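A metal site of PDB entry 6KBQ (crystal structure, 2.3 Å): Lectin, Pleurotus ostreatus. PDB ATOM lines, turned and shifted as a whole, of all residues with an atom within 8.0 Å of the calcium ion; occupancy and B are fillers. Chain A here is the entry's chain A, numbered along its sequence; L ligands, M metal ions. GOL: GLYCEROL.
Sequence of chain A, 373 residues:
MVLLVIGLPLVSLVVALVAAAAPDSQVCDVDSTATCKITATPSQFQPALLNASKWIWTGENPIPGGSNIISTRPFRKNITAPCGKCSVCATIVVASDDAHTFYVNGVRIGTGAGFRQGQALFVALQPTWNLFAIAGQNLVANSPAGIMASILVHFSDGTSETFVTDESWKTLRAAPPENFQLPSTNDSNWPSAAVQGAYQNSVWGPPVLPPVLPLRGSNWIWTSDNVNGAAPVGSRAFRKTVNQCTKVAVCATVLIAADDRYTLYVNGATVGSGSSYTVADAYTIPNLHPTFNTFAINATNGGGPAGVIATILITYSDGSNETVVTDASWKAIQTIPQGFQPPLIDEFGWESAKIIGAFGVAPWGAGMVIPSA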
ATOM      1  N   TRP A  57      15.052  14.895 -19.893  1.00  0.00           N
ATOM      2  CA  TRP A  57      15.892  13.741 -20.153  1.00  0.00           C
ATOM      3  C   TRP A  57      16.215  13.774 -21.633  1.00  0.00           C
ATOM      4  O   TRP A  57      16.155  14.851 -22.248  1.00  0.00           O
ATOM      5  CB  TRP A  57      15.206  12.411 -19.751  1.00  0.00           C
ATOM      6  CG  TRP A  57      16.185  11.271 -19.584  1.00  0.00           C
ATOM      7  CD1 TRP A  57      16.237  10.099 -20.315  1.00  0.00           C
ATOM      8  CD2 TRP A  57      17.294  11.193 -18.655  1.00  0.00           C
ATOM      9  NE1 TRP A  57      17.282   9.316 -19.880  1.00  0.00           N
ATOM     10  CE2 TRP A  57      17.951   9.965 -18.876  1.00  0.00           C
ATOM     11  CE3 TRP A  57      17.777  12.052 -17.657  1.00  0.00           C
ATOM     12  CZ2 TRP A  57      19.065   9.572 -18.124  1.00  0.00           C
ATOM     13  CZ3 TRP A  57      18.892  11.663 -16.915  1.00  0.00           C
ATOM     14  CH2 TRP A  57      19.521  10.429 -17.152  1.00  0.00           C
ATOM     15  N   GLY A  66       8.461   7.687 -19.141  1.00  0.00           N
ATOM     16  CA  GLY A  66       8.484   6.295 -19.512  1.00  0.00           C
ATOM     17  C   GLY A  66       9.764   5.613 -19.044  1.00  0.00           C
ATOM     18  O   GLY A  66      10.678   6.224 -18.478  1.00  0.00           O
ATOM     19  N   ASN A  68      13.288   3.917 -18.951  1.00  0.00           N
ATOM     20  CA  ASN A  68      14.557   4.228 -19.585  1.00  0.00           C
ATOM     21  C   ASN A  68      15.600   3.246 -19.076  1.00  0.00           C
ATOM     22  O   ASN A  68      15.417   2.600 -18.041  1.00  0.00           O
ATOM     23  CB  ASN A  68      14.991   5.659 -19.278  1.00  0.00           C
ATOM     24  CG  ASN A  68      14.207   6.685 -20.087  1.00  0.00           C
ATOM     25  OD1 ASN A  68      13.068   7.052 -19.739  1.00  0.00           O
ATOM     26  ND2 ASN A  68      14.802   7.138 -21.165  1.00  0.00           N
ATOM     27  N   ILE A  69      16.690   3.136 -19.829  1.00  0.00           N
ATOM     28  CA  ILE A  69      17.757   2.216 -19.477  1.00  0.00           C
ATOM     29  C   ILE A  69      18.663   2.850 -18.426  1.00  0.00           C
ATOM     30  O   ILE A  69      18.715   4.079 -18.266  1.00  0.00           O
ATOM     31  CB  ILE A  69      18.581   1.813 -20.717  1.00  0.00           C
ATOM     32  CG1 ILE A  69      19.257   3.060 -21.302  1.00  0.00           C
ATOM     33  CG2 ILE A  69      17.684   1.118 -21.752  1.00  0.00           C
ATOM     34  CD1 ILE A  69      20.351   2.729 -22.344  1.00  0.00           C
ATOM     35  N   ILE A  70      19.422   2.003 -17.724  1.00  0.00           N
ATOM     36  CA  ILE A  70      20.516   2.489 -16.902  1.00  0.00           C
ATOM     37  C   ILE A  70      21.529   3.191 -17.808  1.00  0.00           C
ATOM     38  O   ILE A  70      21.973   2.635 -18.819  1.00  0.00           O
ATOM     39  CB  ILE A  70      21.164   1.343 -16.115  1.00  0.00           C
ATOM     40  CG1 ILE A  70      20.140   0.760 -15.133  1.00  0.00           C
ATOM     41  CG2 ILE A  70      22.415   1.839 -15.363  1.00  0.00           C
ATOM     42  CD1 ILE A  70      20.453  -0.647 -14.649  1.00  0.00           C
ATOM     43  N   SER A  96      16.645  15.042  -9.056  1.00  0.00           N
ATOM     44  CA  SER A  96      17.011  14.081 -10.084  1.00  0.00           C
ATOM     45  C   SER A  96      16.390  12.724  -9.831  1.00  0.00           C
ATOM     46  O   SER A  96      16.242  12.285  -8.688  1.00  0.00           O
ATOM     47  CB  SER A  96      18.533  13.903 -10.181  1.00  0.00           C
ATOM     48  OG  SER A  96      19.047  13.470  -8.924  1.00  0.00           O
ATOM     49  N   ASP A  97      16.072  12.040 -10.922  1.00  0.00           N
ATOM     50  CA  ASP A  97      15.777  10.624 -10.901  1.00  0.00           C
ATOM     51  C   ASP A  97      16.763  10.006 -11.885  1.00  0.00           C
ATOM     52  O   ASP A  97      16.555  10.122 -13.096  1.00  0.00           O
ATOM     53  CB  ASP A  97      14.323  10.365 -11.285  1.00  0.00           C
ATOM     54  CG  ASP A  97      13.975   8.883 -11.321  1.00  0.00           C
ATOM     55  OD1 ASP A  97      14.900   8.055 -11.193  1.00  0.00           O
ATOM     56  OD2 ASP A  97      12.783   8.549 -11.475  1.00  0.00           O
ATOM     57  N   ASP A  98      17.837   9.374 -11.389  1.00  0.00           N
ATOM     58  CA  ASP A  98      18.059   9.070  -9.954  1.00  0.00           C
ATOM     59  C   ASP A  98      19.102   9.945  -9.244  1.00  0.00           C
ATOM     60  O   ASP A  98      19.021  10.145  -8.045  1.00  0.00           O
ATOM     61  CB  ASP A  98      18.514   7.606  -9.782  1.00  0.00           C
ATOM     62  CG  ASP A  98      17.468   6.598 -10.221  1.00  0.00           C
ATOM     63  OD1 ASP A  98      16.615   6.206  -9.392  1.00  0.00           O
ATOM     64  OD2 ASP A  98      17.513   6.165 -11.398  1.00  0.00           O
ATOM     65  N   ALA A  99      20.114  10.434  -9.972  1.00  0.00           N
ATOM     66  CA  ALA A  99      21.242  11.114  -9.356  1.00  0.00           C
ATOM     67  C   ALA A  99      21.801  12.134 -10.331  1.00  0.00           C
ATOM     68  O   ALA A  99      21.579  12.039 -11.540  1.00  0.00           O
ATOM     69  CB  ALA A  99      22.355  10.126  -8.943  1.00  0.00           C
ATOM     70  N   PHE A 115      14.283  12.645  -6.095  1.00  0.00           N
ATOM     71  CA  PHE A 115      13.264  13.546  -6.617  1.00  0.00           C
ATOM     72  C   PHE A 115      12.219  13.954  -5.592  1.00  0.00           C
ATOM     73  O   PHE A 115      11.391  14.823  -5.892  1.00  0.00           O
ATOM     74  CB  PHE A 115      12.564  12.898  -7.823  1.00  0.00           C
ATOM     75  CG  PHE A 115      11.917  11.547  -7.515  1.00  0.00           C
ATOM     76  CD1 PHE A 115      10.606  11.489  -7.034  1.00  0.00           C
ATOM     77  CD2 PHE A 115      12.605  10.359  -7.748  1.00  0.00           C
ATOM     78  CE1 PHE A 115      10.012  10.254  -6.778  1.00  0.00           C
ATOM     79  CE2 PHE A 115      12.020   9.133  -7.487  1.00  0.00           C
ATOM     80  CZ  PHE A 115      10.728   9.072  -6.995  1.00  0.00           C
ATOM     81  N   GLN A 137      21.951  10.597 -14.057  1.00  0.00           N
ATOM     82  CA  GLN A 137      22.099   9.147 -14.135  1.00  0.00           C
ATOM     83  C   GLN A 137      20.779   8.466 -13.808  1.00  0.00           C
ATOM     84  O   GLN A 137      20.178   8.742 -12.762  1.00  0.00           O
ATOM     85  CB  GLN A 137      23.135   8.590 -13.156  1.00  0.00           C
ATOM     86  CG  GLN A 137      24.529   9.190 -13.194  1.00  0.00           C
ATOM     87  CD  GLN A 137      25.339   8.708 -11.978  1.00  0.00           C
ATOM     88  OE1 GLN A 137      25.330   7.516 -11.654  1.00  0.00           O
ATOM     89  NE2 GLN A 137      26.022   9.636 -11.297  1.00  0.00           N
ATOM     90  N   ASN A 138      20.365   7.564 -14.676  1.00  0.00           N
ATOM     91  CA  ASN A 138      19.304   6.620 -14.359  1.00  0.00           C
ATOM     92  C   ASN A 138      19.949   5.349 -13.807  1.00  0.00           C
ATOM     93  O   ASN A 138      20.821   4.759 -14.456  1.00  0.00           O
ATOM     94  CB  ASN A 138      18.467   6.317 -15.595  1.00  0.00           C
ATOM     95  CG  ASN A 138      17.240   5.518 -15.259  1.00  0.00           C
ATOM     96  OD1 ASN A 138      16.777   5.550 -14.114  1.00  0.00           O
ATOM     97  ND2 ASN A 138      16.721   4.766 -16.232  1.00  0.00           N
ATOM     98  N   LEU A 139      19.532   4.941 -12.606  1.00  0.00           N
ATOM     99  CA  LEU A 139      20.210   3.849 -11.935  1.00  0.00           C
ATOM    100  C   LEU A 139      19.378   2.590 -11.810  1.00  0.00           C
ATOM    101  O   LEU A 139      19.920   1.557 -11.410  1.00  0.00           O
ATOM    102  CB  LEU A 139      20.676   4.293 -10.534  1.00  0.00           C
ATOM    103  CG  LEU A 139      21.784   5.353 -10.539  1.00  0.00           C
ATOM    104  CD1 LEU A 139      22.036   5.917  -9.145  1.00  0.00           C
ATOM    105  CD2 LEU A 139      23.090   4.789 -11.107  1.00  0.00           C
ATOM    106  N   VAL A 140      18.094   2.623 -12.156  1.00  0.00           N
ATOM    107  CA  VAL A 140      17.226   1.459 -12.101  1.00  0.00           C
ATOM    108  C   VAL A 140      16.726   1.166 -13.502  1.00  0.00           C
ATOM    109  O   VAL A 140      16.236   2.073 -14.198  1.00  0.00           O
ATOM    110  CB  VAL A 140      16.051   1.687 -11.136  1.00  0.00           C
ATOM    111  CG1 VAL A 140      15.149   0.466 -11.131  1.00  0.00           C
ATOM    112  CG2 VAL A 140      16.560   1.989  -9.730  1.00  0.00           C
ATOM    113  N   ALA A 141      16.831  -0.096 -13.928  1.00  0.00           N
ATOM    114  CA  ALA A 141      16.408  -0.465 -15.270  1.00  0.00           C
ATOM    115  C   ALA A 141      14.892  -0.336 -15.426  1.00  0.00           C
ATOM    116  O   ALA A 141      14.132  -0.524 -14.473  1.00  0.00           O
ATOM    117  CB  ALA A 141      16.849  -1.899 -15.581  1.00  0.00           C
ATOM    118  N   ASN A 142      14.447   0.015 -16.638  1.00  0.00           N
ATOM    119  CA  ASN A 142      13.017   0.113 -16.956  1.00  0.00           C
ATOM    120  C   ASN A 142      12.294   1.149 -16.101  1.00  0.00           C
ATOM    121  O   ASN A 142      11.097   1.041 -15.854  1.00  0.00           O
ATOM    122  CB  ASN A 142      12.285  -1.232 -16.796  1.00  0.00           C
ATOM    123  CG  ASN A 142      12.913  -2.339 -17.581  1.00  0.00           C
ATOM    124  OD1 ASN A 142      13.224  -2.175 -18.771  1.00  0.00           O
ATOM    125  ND2 ASN A 142      13.133  -3.473 -16.936  1.00  0.00           N
ATOM    126  N   SER A 143      13.012   2.147 -15.594  1.00  0.00           N
ATOM    127  CA  SER A 143      12.406   3.116 -14.693  1.00  0.00           C
ATOM    128  C   SER A 143      12.507   4.506 -15.294  1.00  0.00           C
ATOM    129  O   SER A 143      13.358   4.762 -16.164  1.00  0.00           O
ATOM    130  CB  SER A 143      13.110   3.076 -13.328  1.00  0.00           C
ATOM    131  OG  SER A 143      14.320   3.810 -13.375  1.00  0.00           O
ATOM    132  N   PRO A 144      11.665   5.447 -14.856  1.00  0.00           N
ATOM    133  CA  PRO A 144      11.743   6.806 -15.418  1.00  0.00           C
ATOM    134  C   PRO A 144      13.081   7.459 -15.094  1.00  0.00           C
ATOM    135  O   PRO A 144      13.833   7.017 -14.219  1.00  0.00           O
ATOM    136  CB  PRO A 144      10.574   7.547 -14.757  1.00  0.00           C
ATOM    137  CG  PRO A 144      10.089   6.686 -13.659  1.00  0.00           C
ATOM    138  CD  PRO A 144      10.536   5.271 -13.939  1.00  0.00           C
ATOM    139  N   ALA A 145      13.396   8.512 -15.843  1.00  0.00           N
ATOM    140  CA  ALA A 145      14.645   9.256 -15.661  1.00  0.00           C
ATOM    141  C   ALA A 145      14.388  10.736 -15.909  1.00  0.00           C
ATOM    142  O   ALA A 145      13.599  11.091 -16.795  1.00  0.00           O
ATOM    143  CB  ALA A 145      15.744   8.745 -16.597  1.00  0.00           C
ATOM    144  N   GLY A 146      15.055  11.594 -15.151  1.00  0.00           N
ATOM    145  CA  GLY A 146      14.898  13.019 -15.382  1.00  0.00           C
ATOM    146  C   GLY A 146      15.643  13.871 -14.378  1.00  0.00           C
ATOM    147  O   GLY A 146      15.991  13.419 -13.276  1.00  0.00           O
ATOM    148  N   TRP A 204       6.688  12.168 -11.090  1.00  0.00           N
ATOM    149  CA  TRP A 204       7.342  12.366  -9.797  1.00  0.00           C
ATOM    150  C   TRP A 204       6.510  13.163  -8.796  1.00  0.00           C
ATOM    151  O   TRP A 204       6.740  13.021  -7.595  1.00  0.00           O
ATOM    152  CB  TRP A 204       8.691  13.069 -10.023  1.00  0.00           C
ATOM    153  CG  TRP A 204       9.569  12.213 -10.860  1.00  0.00           C
ATOM    154  CD1 TRP A 204      10.235  11.070 -10.468  1.00  0.00           C
ATOM    155  CD2 TRP A 204       9.850  12.382 -12.260  1.00  0.00           C
ATOM    156  NE1 TRP A 204      10.926  10.536 -11.537  1.00  0.00           N
ATOM    157  CE2 TRP A 204      10.701  11.308 -12.647  1.00  0.00           C
ATOM    158  CE3 TRP A 204       9.476  13.331 -13.224  1.00  0.00           C
ATOM    159  CZ2 TRP A 204      11.182  11.172 -13.949  1.00  0.00           C
ATOM    160  CZ3 TRP A 204       9.955  13.186 -14.508  1.00  0.00           C
ATOM    161  CH2 TRP A 204      10.802  12.119 -14.860  1.00  0.00           C
HETATM  162  C1  GOL L   1      11.201   5.502  -9.751  1.00  0.00           C
HETATM  163  O1  GOL L   1      11.181   5.144  -8.405  1.00  0.00           O
HETATM  164  C2  GOL L   1      12.680   5.763 -10.146  1.00  0.00           C
HETATM  165  O2  GOL L   1      12.848   5.899 -11.515  1.00  0.00           O
HETATM  166  C3  GOL L   1      13.528   4.597  -9.551  1.00  0.00           C
HETATM  167  O3  GOL L   1      14.792   4.657 -10.167  1.00  0.00           O
HETATM  168 CA    CA M   1      15.133   6.053 -12.422  1.00  0.00          CA
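The calcium ion is bound by OD1 of Asp 97, OD1 of Asn 138, O of Pro 144, O2 of the ligand, OG of Ser 143, OD2 of Asp 98 and O3 of the ligand.
The backbone NH of Asp 97 sits at hydrogen-bond distance from the backbone carbonyl oxygen of Gly 146 (2.7 Å).
The indole nitrogen (NE1) of Trp 204 sits at hydrogen-bond distance from the side-chain carboxylate (OD2) of Asp 97, 2.7 Å away.
The backbone carbonyl oxygen of Val 140 lies within hydrogen-bond range of the side-chain amide nitrogen of Asn 138 (3.4 Å).
The side-chain amide nitrogen of Asn 138 lies within hydrogen-bond range of the backbone carbonyl oxygen of Asn 68, 3.1 Å away.
The side-chain hydroxyl (OG) of Ser 143 sits close to the backbone carbonyl oxygen (O) of Val 140, 2.7 Å away.
O of Ser 143 sits at hydrogen-bond distance from N of Asn 68 (2.9 Å).
The backbone carbonyl oxygen (O) of Gln 137 sits at hydrogen-bond distance from the backbone NH (N) of Asp 98 (2.8 Å).
The backbone carbonyl oxygen (O) of Asp 98 sits at hydrogen-bond distance from the side-chain hydroxyl (OG) of Ser 96 (3.4 Å).
The nearest printed residue that does not touch the calcium ion is Val 140 (4.5 Å).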
